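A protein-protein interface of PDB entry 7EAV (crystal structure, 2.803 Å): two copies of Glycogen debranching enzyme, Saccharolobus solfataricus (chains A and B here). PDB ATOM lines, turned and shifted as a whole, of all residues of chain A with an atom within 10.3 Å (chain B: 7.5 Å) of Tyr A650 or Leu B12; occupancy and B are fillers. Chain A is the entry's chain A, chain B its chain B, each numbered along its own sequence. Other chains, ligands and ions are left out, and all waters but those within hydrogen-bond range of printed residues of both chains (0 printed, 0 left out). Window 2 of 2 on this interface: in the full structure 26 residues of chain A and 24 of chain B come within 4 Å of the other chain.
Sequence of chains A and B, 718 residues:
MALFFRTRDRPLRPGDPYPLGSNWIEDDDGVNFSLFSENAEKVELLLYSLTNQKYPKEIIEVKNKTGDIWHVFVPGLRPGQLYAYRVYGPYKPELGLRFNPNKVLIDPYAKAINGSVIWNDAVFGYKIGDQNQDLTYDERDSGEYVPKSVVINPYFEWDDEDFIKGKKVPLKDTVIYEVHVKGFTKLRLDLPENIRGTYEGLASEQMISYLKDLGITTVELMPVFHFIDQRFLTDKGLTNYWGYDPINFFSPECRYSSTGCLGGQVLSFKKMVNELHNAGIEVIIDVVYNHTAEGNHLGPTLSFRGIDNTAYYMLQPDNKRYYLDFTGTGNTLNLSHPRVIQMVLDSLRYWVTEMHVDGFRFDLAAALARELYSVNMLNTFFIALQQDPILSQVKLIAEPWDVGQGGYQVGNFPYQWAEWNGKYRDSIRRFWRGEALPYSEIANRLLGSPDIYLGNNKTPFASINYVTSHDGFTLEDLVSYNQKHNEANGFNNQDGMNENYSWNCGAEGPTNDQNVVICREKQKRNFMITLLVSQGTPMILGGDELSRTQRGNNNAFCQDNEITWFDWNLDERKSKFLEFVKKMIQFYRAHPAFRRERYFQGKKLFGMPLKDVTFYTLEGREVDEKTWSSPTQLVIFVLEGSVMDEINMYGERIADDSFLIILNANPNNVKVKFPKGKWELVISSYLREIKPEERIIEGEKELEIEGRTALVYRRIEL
Among the printed residues, pairs that only touch across the chains: Asn A648 with Pro B14, Met A649 with Arg B13, Met A649 with Pro B14, Tyr A650 with Leu B12, Tyr A650 with Arg B13, Gly A651 with Leu B12 and Gly A651 with Pro B14.
No position is printed for both chains.
Of the 12 printed residues of chain A, 4 touch a printed residue of chain B.
Printed residues of chain A that touch a printed residue of chain B: Asn A648, Met A649, Tyr A650 and Gly A651.
Hydrophobic or aromatic side chains of chain A that line the printed part of chain B: Tyr A650.
Along chain A the printed residues that touch a printed residue of chain B span positions 648 to 651.
Of the 22 printed residues of chain B, 3 touch a printed residue of chain A.
Hydrophobic or aromatic side chains of chain B that line the printed part of chain A: Pro B14.
Among the printed residues, 7 pairs touch across the chains.
The backbone NH (N) of Arg B13 sits at hydrogen-bond distance from the backbone carbonyl oxygen (O) of Phe B73.
The guanidinium group (NH1) of Arg B13 is in salt-bridge range of the side-chain carboxylate (OD2) of Asp B28 (3.0 Å).
The backbone NH (N) of Gly A651 is in hydrogen-bond range of the side-chain amide oxygen (OD1) of Asn A648.
The side-chain amide nitrogen of Asn A648 lies within hydrogen-bond range of the side-chain carboxylate of Glu A652 (2.9 Å).
The side-chain amide oxygen of Asn A648 lies close to the backbone NH of Tyr A650, 3.1 Å away.
Lys A172 touches none of the printed residues of chain B.
Printed residues of chain B within 4 Å of Asn A648: Pro B14 (3.2 Å).
Of the printed residues of chain B, Tyr A650 touches Leu B12 and Arg B13.
No residue of chain A comes within 4 Å of Arg B10.
No residue of chain A comes within 4 Å of Pro B11.
Leu B12 touches just these residues of chain A: Tyr A650 and Gly A651.
Of the printed residues of chain A, Pro B14 touches Asn A648, Met A649 and Gly A651.
Glu B61 touches none of the printed residues of chain A.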
ATOM      1  N   LYS A 167      19.366 -18.826  43.264  1.00  0.00           N
ATOM      2  CA  LYS A 167      20.602 -18.997  42.594  1.00  0.00           C
ATOM      3  C   LYS A 167      21.561 -19.051  43.724  1.00  0.00           C
ATOM      4  O   LYS A 167      22.104 -18.055  44.130  1.00  0.00           O
ATOM      5  CB  LYS A 167      20.849 -17.863  41.624  1.00  0.00           C
ATOM      6  CG  LYS A 167      20.209 -18.160  40.280  1.00  0.00           C
ATOM      7  CD  LYS A 167      19.473 -16.978  39.667  1.00  0.00           C
ATOM      8  CE  LYS A 167      18.512 -16.295  40.621  1.00  0.00           C
ATOM      9  NZ  LYS A 167      17.088 -16.613  40.341  1.00  0.00           N
ATOM     10  N   LYS A 172      28.055 -24.927  38.124  1.00  0.00           N
ATOM     11  CA  LYS A 172      29.170 -24.395  37.351  1.00  0.00           C
ATOM     12  C   LYS A 172      30.375 -24.099  38.240  1.00  0.00           C
ATOM     13  O   LYS A 172      31.500 -24.506  37.935  1.00  0.00           O
ATOM     14  CB  LYS A 172      28.707 -23.138  36.613  1.00  0.00           C
ATOM     15  CG  LYS A 172      29.763 -22.441  35.789  1.00  0.00           C
ATOM     16  CD  LYS A 172      29.129 -21.366  34.918  1.00  0.00           C
ATOM     17  CE  LYS A 172      28.312 -20.391  35.754  1.00  0.00           C
ATOM     18  NZ  LYS A 172      29.177 -19.427  36.491  1.00  0.00           N
ATOM     19  N   GLU A 597      30.088 -24.089  31.246  1.00  0.00           N
ATOM     20  CA  GLU A 597      28.825 -24.778  31.030  1.00  0.00           C
ATOM     21  C   GLU A 597      28.800 -25.546  29.714  1.00  0.00           C
ATOM     22  O   GLU A 597      27.982 -26.458  29.554  1.00  0.00           O
ATOM     23  CB  GLU A 597      27.665 -23.772  31.092  1.00  0.00           C
ATOM     24  CG  GLU A 597      26.275 -24.366  30.874  1.00  0.00           C
ATOM     25  CD  GLU A 597      25.203 -23.662  31.683  1.00  0.00           C
ATOM     26  OE1 GLU A 597      24.068 -24.182  31.746  1.00  0.00           O
ATOM     27  OE2 GLU A 597      25.495 -22.593  32.259  1.00  0.00           O
ATOM     28  N   GLU A 646      31.261 -19.475  25.946  1.00  0.00           N
ATOM     29  CA  GLU A 646      30.723 -19.494  27.298  1.00  0.00           C
ATOM     30  C   GLU A 646      29.820 -18.285  27.490  1.00  0.00           C
ATOM     31  O   GLU A 646      30.282 -17.143  27.400  1.00  0.00           O
ATOM     32  CB  GLU A 646      31.847 -19.490  28.334  1.00  0.00           C
ATOM     33  CG  GLU A 646      31.987 -20.789  29.095  1.00  0.00           C
ATOM     34  CD  GLU A 646      30.656 -21.333  29.568  1.00  0.00           C
ATOM     35  OE1 GLU A 646      29.999 -20.667  30.396  1.00  0.00           O
ATOM     36  OE2 GLU A 646      30.264 -22.426  29.109  1.00  0.00           O
ATOM     37  N   ILE A 647      28.544 -18.539  27.764  1.00  0.00           N
ATOM     38  CA  ILE A 647      27.542 -17.496  27.948  1.00  0.00           C
ATOM     39  C   ILE A 647      27.025 -17.573  29.378  1.00  0.00           C
ATOM     40  O   ILE A 647      26.678 -18.659  29.858  1.00  0.00           O
ATOM     41  CB  ILE A 647      26.383 -17.643  26.943  1.00  0.00           C
ATOM     42  CG1 ILE A 647      26.921 -18.014  25.559  1.00  0.00           C
ATOM     43  CG2 ILE A 647      25.560 -16.366  26.880  1.00  0.00           C
ATOM     44  CD1 ILE A 647      27.567 -16.859  24.830  1.00  0.00           C
ATOM     45  N   ASN A 648      26.981 -16.430  30.058  1.00  0.00           N
ATOM     46  CA  ASN A 648      26.390 -16.373  31.386  1.00  0.00           C
ATOM     47  C   ASN A 648      24.881 -16.169  31.280  1.00  0.00           C
ATOM     48  O   ASN A 648      24.328 -15.969  30.196  1.00  0.00           O
ATOM     49  CB  ASN A 648      27.042 -15.273  32.233  1.00  0.00           C
ATOM     50  CG  ASN A 648      26.969 -13.895  31.589  1.00  0.00           C
ATOM     51  OD1 ASN A 648      26.013 -13.563  30.888  1.00  0.00           O
ATOM     52  ND2 ASN A 648      27.987 -13.079  31.839  1.00  0.00           N
ATOM     53  N   MET A 649      24.210 -16.211  32.433  1.00  0.00           N
ATOM     54  CA  MET A 649      22.752 -16.167  32.458  1.00  0.00           C
ATOM     55  C   MET A 649      22.178 -14.844  31.962  1.00  0.00           C
ATOM     56  O   MET A 649      20.957 -14.747  31.798  1.00  0.00           O
ATOM     57  CB  MET A 649      22.243 -16.451  33.874  1.00  0.00           C
ATOM     58  CG  MET A 649      22.778 -15.508  34.935  1.00  0.00           C
ATOM     59  SD  MET A 649      21.988 -15.761  36.536  1.00  0.00           S
ATOM     60  CE  MET A 649      20.339 -15.144  36.202  1.00  0.00           C
ATOM     61  N   TYR A 650      23.012 -13.834  31.715  1.00  0.00           N
ATOM     62  CA  TYR A 650      22.555 -12.552  31.197  1.00  0.00           C
ATOM     63  C   TYR A 650      22.794 -12.402  29.700  1.00  0.00           C
ATOM     64  O   TYR A 650      22.587 -11.312  29.159  1.00  0.00           O
ATOM     65  CB  TYR A 650      23.234 -11.404  31.947  1.00  0.00           C
ATOM     66  CG  TYR A 650      23.026 -11.442  33.443  1.00  0.00           C
ATOM     67  CD1 TYR A 650      21.910 -10.854  34.023  1.00  0.00           C
ATOM     68  CD2 TYR A 650      23.942 -12.072  34.275  1.00  0.00           C
ATOM     69  CE1 TYR A 650      21.713 -10.888  35.391  1.00  0.00           C
ATOM     70  CE2 TYR A 650      23.755 -12.110  35.644  1.00  0.00           C
ATOM     71  CZ  TYR A 650      22.639 -11.518  36.196  1.00  0.00           C
ATOM     72  OH  TYR A 650      22.448 -11.555  37.558  1.00  0.00           O
ATOM     73  N   GLY A 651      23.223 -13.461  29.021  1.00  0.00           N
ATOM     74  CA  GLY A 651      23.457 -13.384  27.595  1.00  0.00           C
ATOM     75  C   GLY A 651      24.787 -12.794  27.188  1.00  0.00           C
ATOM     76  O   GLY A 651      25.007 -12.575  25.992  1.00  0.00           O
ATOM     77  N   GLU A 652      25.677 -12.519  28.137  1.00  0.00           N
ATOM     78  CA  GLU A 652      27.020 -12.063  27.816  1.00  0.00           C
ATOM     79  C   GLU A 652      27.927 -13.262  27.596  1.00  0.00           C
ATOM     80  O   GLU A 652      27.833 -14.267  28.309  1.00  0.00           O
ATOM     81  CB  GLU A 652      27.597 -11.198  28.938  1.00  0.00           C
ATOM     82  CG  GLU A 652      26.707 -10.071  29.407  1.00  0.00           C
ATOM     83  CD  GLU A 652      27.210  -9.444  30.693  1.00  0.00           C
ATOM     84  OE1 GLU A 652      27.486 -10.194  31.654  1.00  0.00           O
ATOM     85  OE2 GLU A 652      27.335  -8.204  30.744  1.00  0.00           O
ATOM     86  N   ARG A 653      28.808 -13.159  26.608  1.00  0.00           N
ATOM     87  CA  ARG A 653      29.857 -14.155  26.537  1.00  0.00           C
ATOM     88  C   ARG A 653      30.889 -13.873  27.626  1.00  0.00           C
ATOM     89  O   ARG A 653      30.906 -12.805  28.244  1.00  0.00           O
ATOM     90  CB  ARG A 653      30.501 -14.180  25.152  1.00  0.00           C
ATOM     91  CG  ARG A 653      31.268 -15.464  24.873  1.00  0.00           C
ATOM     92  CD  ARG A 653      31.772 -15.542  23.453  1.00  0.00           C
ATOM     93  NE  ARG A 653      32.256 -14.268  22.939  1.00  0.00           N
ATOM     94  CZ  ARG A 653      33.490 -14.071  22.488  1.00  0.00           C
ATOM     95  NH1 ARG A 653      34.371 -15.063  22.511  1.00  0.00           N
ATOM     96  NH2 ARG A 653      33.850 -12.881  22.030  1.00  0.00           N
ATOM     97  N   ILE A 654      31.744 -14.856  27.880  1.00  0.00           N
ATOM     98  CA  ILE A 654      32.730 -14.787  28.946  1.00  0.00           C
ATOM     99  C   ILE A 654      34.115 -14.959  28.344  1.00  0.00           C
ATOM    100  O   ILE A 654      34.322 -15.809  27.470  1.00  0.00           O
ATOM    101  CB  ILE A 654      32.456 -15.854  30.024  1.00  0.00           C
ATOM    102  CG1 ILE A 654      31.360 -15.371  30.971  1.00  0.00           C
ATOM    103  CG2 ILE A 654      33.721 -16.181  30.794  1.00  0.00           C
ATOM    104  CD1 ILE A 654      31.072 -16.318  32.102  1.00  0.00           C
ATOM    105  N   THR B   7      19.987 -13.425  14.261  1.00  0.00           N
ATOM    106  CA  THR B   7      19.342 -13.676  15.545  1.00  0.00           C
ATOM    107  C   THR B   7      20.179 -13.222  16.738  1.00  0.00           C
ATOM    108  O   THR B   7      19.667 -13.143  17.860  1.00  0.00           O
ATOM    109  CB  THR B   7      19.027 -15.169  15.672  1.00  0.00           C
ATOM    110  OG1 THR B   7      18.038 -15.372  16.688  1.00  0.00           O
ATOM    111  CG2 THR B   7      20.287 -15.955  16.015  1.00  0.00           C
ATOM    112  N   ARG B   8      21.459 -12.924  16.517  1.00  0.00           N
ATOM    113  CA  ARG B   8      22.352 -12.514  17.592  1.00  0.00           C
ATOM    114  C   ARG B   8      22.402 -11.006  17.798  1.00  0.00           C
ATOM    115  O   ARG B   8      23.040 -10.552  18.754  1.00  0.00           O
ATOM    116  CB  ARG B   8      23.771 -13.028  17.327  1.00  0.00           C
ATOM    117  CG  ARG B   8      24.497 -12.339  16.178  1.00  0.00           C
ATOM    118  CD  ARG B   8      25.964 -12.732  16.174  1.00  0.00           C
ATOM    119  NE  ARG B   8      26.145 -14.076  16.714  1.00  0.00           N
ATOM    120  CZ  ARG B   8      27.199 -14.467  17.423  1.00  0.00           C
ATOM    121  NH1 ARG B   8      28.178 -13.613  17.682  1.00  0.00           N
ATOM    122  NH2 ARG B   8      27.272 -15.711  17.876  1.00  0.00           N
ATOM    123  N   ASP B   9      21.757 -10.223  16.937  1.00  0.00           N
ATOM    124  CA  ASP B   9      21.783  -8.772  17.050  1.00  0.00           C
ATOM    125  C   ASP B   9      20.553  -8.205  17.745  1.00  0.00           C
ATOM    126  O   ASP B   9      20.440  -6.982  17.871  1.00  0.00           O
ATOM    127  CB  ASP B   9      21.945  -8.135  15.667  1.00  0.00           C
ATOM    128  CG  ASP B   9      23.210  -8.591  14.966  1.00  0.00           C
ATOM    129  OD1 ASP B   9      24.312  -8.257  15.454  1.00  0.00           O
ATOM    130  OD2 ASP B   9      23.105  -9.289  13.937  1.00  0.00           O
ATOM    131  N   ARG B  10      19.630  -9.052  18.190  1.00  0.00           N
ATOM    132  CA  ARG B  10      18.593  -8.601  19.100  1.00  0.00           C
ATOM    133  C   ARG B  10      18.855  -9.187  20.479  1.00  0.00           C
ATOM    134  O   ARG B  10      19.149 -10.385  20.590  1.00  0.00           O
ATOM    135  CB  ARG B  10      17.193  -8.992  18.595  1.00  0.00           C
ATOM    136  CG  ARG B  10      16.913 -10.478  18.476  1.00  0.00           C
ATOM    137  CD  ARG B  10      16.052 -10.952  19.634  1.00  0.00           C
ATOM    138  NE  ARG B  10      14.691 -10.425  19.565  1.00  0.00           N
ATOM    139  CZ  ARG B  10      14.196  -9.515  20.397  1.00  0.00           C
ATOM    140  NH1 ARG B  10      14.950  -9.019  21.371  1.00  0.00           N
ATOM    141  NH2 ARG B  10      12.944  -9.096  20.259  1.00  0.00           N
ATOM    142  N   PRO B  11      18.798  -8.377  21.536  1.00  0.00           N
ATOM    143  CA  PRO B  11      19.294  -8.831  22.843  1.00  0.00           C
ATOM    144  C   PRO B  11      18.498 -10.015  23.372  1.00  0.00           C
ATOM    145  O   PRO B  11      17.271 -10.061  23.264  1.00  0.00           O
ATOM    146  CB  PRO B  11      19.128  -7.595  23.737  1.00  0.00           C
ATOM    147  CG  PRO B  11      18.988  -6.439  22.790  1.00  0.00           C
ATOM    148  CD  PRO B  11      18.310  -6.990  21.578  1.00  0.00           C
ATOM    149  N   LEU B  12      19.218 -10.983  23.939  1.00  0.00           N
ATOM    150  CA  LEU B  12      18.607 -12.201  24.452  1.00  0.00           C
ATOM    151  C   LEU B  12      19.384 -12.690  25.666  1.00  0.00           C
ATOM    152  O   LEU B  12      20.527 -12.288  25.904  1.00  0.00           O
ATOM    153  CB  LEU B  12      18.560 -13.308  23.390  1.00  0.00           C
ATOM    154  CG  LEU B  12      17.683 -13.094  22.156  1.00  0.00           C
ATOM    155  CD1 LEU B  12      17.985 -14.144  21.098  1.00  0.00           C
ATOM    156  CD2 LEU B  12      16.212 -13.118  22.538  1.00  0.00           C
ATOM    157  N   ARG B  13      18.741 -13.567  26.432  1.00  0.00           N
ATOM    158  CA  ARG B  13      19.344 -14.306  27.527  1.00  0.00           C
ATOM    159  C   ARG B  13      19.157 -15.802  27.295  1.00  0.00           C
ATOM    160  O   ARG B  13      18.177 -16.216  26.670  1.00  0.00           O
ATOM    161  CB  ARG B  13      18.732 -13.926  28.881  1.00  0.00           C
ATOM    162  CG  ARG B  13      19.030 -12.513  29.365  1.00  0.00           C
ATOM    163  CD  ARG B  13      18.924 -12.451  30.884  1.00  0.00           C
ATOM    164  NE  ARG B  13      18.692 -11.103  31.393  1.00  0.00           N
ATOM    165  CZ  ARG B  13      18.248 -10.840  32.618  1.00  0.00           C
ATOM    166  NH1 ARG B  13      17.987 -11.836  33.455  1.00  0.00           N
ATOM    167  NH2 ARG B  13      18.062  -9.587  33.009  1.00  0.00           N
ATOM    168  N   PRO B  14      20.082 -16.635  27.780  1.00  0.00           N
ATOM    169  CA  PRO B  14      19.939 -18.085  27.560  1.00  0.00           C
ATOM    170  C   PRO B  14      18.676 -18.675  28.164  1.00  0.00           C
ATOM    171  O   PRO B  14      18.152 -19.662  27.633  1.00  0.00           O
ATOM    172  CB  PRO B  14      21.203 -18.669  28.211  1.00  0.00           C
ATOM    173  CG  PRO B  14      21.734 -17.582  29.096  1.00  0.00           C
ATOM    174  CD  PRO B  14      21.354 -16.299  28.438  1.00  0.00           C
ATOM    175  N   GLY B  15      18.166 -18.102  29.250  1.00  0.00           N
ATOM    176  CA  GLY B  15      16.955 -18.607  29.860  1.00  0.00           C
ATOM    177  C   GLY B  15      17.184 -19.878  30.659  1.00  0.00           C
ATOM    178  O   GLY B  15      18.313 -20.322  30.888  1.00  0.00           O
ATOM    179  N   ASP B  28      13.026  -9.374  36.272  1.00  0.00           N
ATOM    180  CA  ASP B  28      14.038  -9.115  35.258  1.00  0.00           C
ATOM    181  C   ASP B  28      13.472  -8.469  34.002  1.00  0.00           C
ATOM    182  O   ASP B  28      14.226  -8.236  33.051  1.00  0.00           O
ATOM    183  CB  ASP B  28      14.765 -10.416  34.894  1.00  0.00           C
ATOM    184  CG  ASP B  28      15.581 -10.972  36.049  1.00  0.00           C
ATOM    185  OD1 ASP B  28      15.584 -10.354  37.135  1.00  0.00           O
ATOM    186  OD2 ASP B  28      16.222 -12.029  35.868  1.00  0.00           O
ATOM    187  N   LEU B  45      10.943 -19.134  17.747  1.00  0.00           N
ATOM    188  CA  LEU B  45       9.891 -18.461  18.497  1.00  0.00           C
ATOM    189  C   LEU B  45       9.284 -17.348  17.650  1.00  0.00           C
ATOM    190  O   LEU B  45      10.007 -16.507  17.107  1.00  0.00           O
ATOM    191  CB  LEU B  45      10.447 -17.892  19.803  1.00  0.00           C
ATOM    192  CG  LEU B  45       9.473 -17.104  20.679  1.00  0.00           C
ATOM    193  CD1 LEU B  45       8.360 -18.005  21.191  1.00  0.00           C
ATOM    194  CD2 LEU B  45      10.211 -16.443  21.834  1.00  0.00           C
ATOM    195  N   LEU B  47       6.637 -14.111  17.438  1.00  0.00           N
ATOM    196  CA  LEU B  47       5.991 -13.080  18.237  1.00  0.00           C
ATOM    197  C   LEU B  47       5.084 -12.257  17.336  1.00  0.00           C
ATOM    198  O   LEU B  47       5.511 -11.797  16.272  1.00  0.00           O
ATOM    199  CB  LEU B  47       7.024 -12.187  18.927  1.00  0.00           C
ATOM    200  CG  LEU B  47       8.091 -12.931  19.733  1.00  0.00           C
ATOM    201  CD1 LEU B  47       9.240 -12.006  20.106  1.00  0.00           C
ATOM    202  CD2 LEU B  47       7.474 -13.558  20.972  1.00  0.00           C
ATOM    203  N   GLU B  58       8.088 -10.741  14.698  1.00  0.00           N
ATOM    204  CA  GLU B  58       9.487 -11.045  14.961  1.00  0.00           C
ATOM    205  C   GLU B  58       9.672 -12.555  15.017  1.00  0.00           C
ATOM    206  O   GLU B  58       8.848 -13.265  15.600  1.00  0.00           O
ATOM    207  CB  GLU B  58       9.964 -10.407  16.271  1.00  0.00           C
ATOM    208  CG  GLU B  58      11.433 -10.656  16.574  1.00  0.00           C
ATOM    209  CD  GLU B  58      12.126  -9.440  17.152  1.00  0.00           C
ATOM    210  OE1 GLU B  58      13.371  -9.370  17.076  1.00  0.00           O
ATOM    211  OE2 GLU B  58      11.426  -8.553  17.682  1.00  0.00           O
ATOM    212  N   ILE B  60      12.415 -15.348  16.316  1.00  0.00           N
ATOM    213  CA  ILE B  60      13.587 -15.621  17.139  1.00  0.00           C
ATOM    214  C   ILE B  60      13.852 -17.117  17.104  1.00  0.00           C
ATOM    215  O   ILE B  60      12.921 -17.922  17.217  1.00  0.00           O
ATOM    216  CB  ILE B  60      13.391 -15.140  18.592  1.00  0.00           C
ATOM    217  CG1 ILE B  60      13.389 -13.616  18.664  1.00  0.00           C
ATOM    218  CG2 ILE B  60      14.477 -15.700  19.501  1.00  0.00           C
ATOM    219  CD1 ILE B  60      12.988 -13.097  20.020  1.00  0.00           C
ATOM    220  N   GLU B  61      15.120 -17.492  16.951  1.00  0.00           N
ATOM    221  CA  GLU B  61      15.518 -18.892  16.909  1.00  0.00           C
ATOM    222  C   GLU B  61      15.958 -19.338  18.297  1.00  0.00           C
ATOM    223  O   GLU B  61      16.935 -18.813  18.843  1.00  0.00           O
ATOM    224  CB  GLU B  61      16.640 -19.119  15.896  1.00  0.00           C
ATOM    225  CG  GLU B  61      16.968 -20.588  15.684  1.00  0.00           C
ATOM    226  CD  GLU B  61      18.356 -20.807  15.117  1.00  0.00           C
ATOM    227  OE1 GLU B  61      18.676 -21.961  14.759  1.00  0.00           O
ATOM    228  OE2 GLU B  61      19.126 -19.828  15.027  1.00  0.00           O
ATOM    229  N   VAL B  62      15.240 -20.308  18.862  1.00  0.00           N
ATOM    230  CA  VAL B  62      15.600 -20.888  20.150  1.00  0.00           C
ATOM    231  C   VAL B  62      16.862 -21.721  19.971  1.00  0.00           C
ATOM    232  O   VAL B  62      16.800 -22.875  19.533  1.00  0.00           O
ATOM    233  CB  VAL B  62      14.454 -21.737  20.726  1.00  0.00           C
ATOM    234  CG1 VAL B  62      14.801 -22.207  22.127  1.00  0.00           C
ATOM    235  CG2 VAL B  62      13.158 -20.946  20.728  1.00  0.00           C
ATOM    236  N   LYS B  63      18.012 -21.141  20.306  1.00  0.00           N
ATOM    237  CA  LYS B  63      19.285 -21.817  20.108  1.00  0.00           C
ATOM    238  C   LYS B  63      19.776 -22.548  21.350  1.00  0.00           C
ATOM    239  O   LYS B  63      20.578 -23.481  21.224  1.00  0.00           O
ATOM    240  CB  LYS B  63      20.347 -20.813  19.653  1.00  0.00           C
ATOM    241  CG  LYS B  63      20.206 -20.390  18.198  1.00  0.00           C
ATOM    242  CD  LYS B  63      21.084 -19.192  17.876  1.00  0.00           C
ATOM    243  CE  LYS B  63      22.557 -19.554  17.953  1.00  0.00           C
ATOM    244  NZ  LYS B  63      23.419 -18.344  18.006  1.00  0.00           N
ATOM    245  N   ASN B  64      19.317 -22.160  22.537  1.00  0.00           N
ATOM    246  CA  ASN B  64      19.761 -22.808  23.762  1.00  0.00           C
ATOM    247  C   ASN B  64      18.935 -24.055  24.043  1.00  0.00           C
ATOM    248  O   ASN B  64      17.708 -24.055  23.900  1.00  0.00           O
ATOM    249  CB  ASN B  64      19.673 -21.843  24.944  1.00  0.00           C
ATOM    250  CG  ASN B  64      20.653 -20.693  24.829  1.00  0.00           C
ATOM    251  OD1 ASN B  64      20.316 -19.622  24.324  1.00  0.00           O
ATOM    252  ND2 ASN B  64      21.876 -20.913  25.296  1.00  0.00           N
ATOM    253  N   VAL B  72      14.600 -19.973  25.672  1.00  0.00           N
ATOM    254  CA  VAL B  72      15.200 -18.662  25.452  1.00  0.00           C
ATOM    255  C   VAL B  72      14.420 -17.654  26.285  1.00  0.00           C
ATOM    256  O   VAL B  72      13.219 -17.815  26.519  1.00  0.00           O
ATOM    257  CB  VAL B  72      15.208 -18.272  23.951  1.00  0.00           C
ATOM    258  CG1 VAL B  72      13.788 -18.153  23.413  1.00  0.00           C
ATOM    259  CG2 VAL B  72      15.986 -16.977  23.725  1.00  0.00           C
ATOM    260  N   PHE B  73      15.117 -16.625  26.759  1.00  0.00           N
ATOM    261  CA  PHE B  73      14.510 -15.533  27.509  1.00  0.00           C
ATOM    262  C   PHE B  73      14.616 -14.265  26.671  1.00  0.00           C
ATOM    263  O   PHE B  73      15.726 -13.804  26.381  1.00  0.00           O
ATOM    264  CB  PHE B  73      15.191 -15.357  28.868  1.00  0.00           C
ATOM    265  CG  PHE B  73      14.807 -14.094  29.590  1.00  0.00           C
ATOM    266  CD1 PHE B  73      13.704 -14.067  30.426  1.00  0.00           C
ATOM    267  CD2 PHE B  73      15.559 -12.938  29.448  1.00  0.00           C
ATOM    268  CE1 PHE B  73      13.355 -12.908  31.095  1.00  0.00           C
ATOM    269  CE2 PHE B  73      15.216 -11.781  30.113  1.00  0.00           C
ATOM    270  CZ  PHE B  73      14.115 -11.765  30.939  1.00  0.00           C
ATOM    271  N   VAL B  74      13.474 -13.712  26.285  1.00  0.00           N
ATOM    272  CA  VAL B  74      13.420 -12.551  25.395  1.00  0.00           C
ATOM    273  C   VAL B  74      13.158 -11.315  26.257  1.00  0.00           C
ATOM    274  O   VAL B  74      12.080 -11.214  26.861  1.00  0.00           O
ATOM    275  CB  VAL B  74      12.343 -12.718  24.317  1.00  0.00           C
ATOM    276  CG1 VAL B  74      12.303 -11.494  23.417  1.00  0.00           C
ATOM    277  CG2 VAL B  74      12.605 -13.978  23.504  1.00  0.00           C
ATOM    278  N   PRO B  75      14.097 -10.377  26.346  1.00  0.00           N
ATOM    279  CA  PRO B  75      13.867  -9.181  27.165  1.00  0.00           C
ATOM    280  C   PRO B  75      12.835  -8.258  26.539  1.00  0.00           C
ATOM    281  O   PRO B  75      12.545  -8.313  25.341  1.00  0.00           O
ATOM    282  CB  PRO B  75      15.246  -8.510  27.219  1.00  0.00           C
ATOM    283  CG  PRO B  75      16.220  -9.562  26.786  1.00  0.00           C
ATOM    284  CD  PRO B  75      15.471 -10.433  25.827  1.00  0.00           C
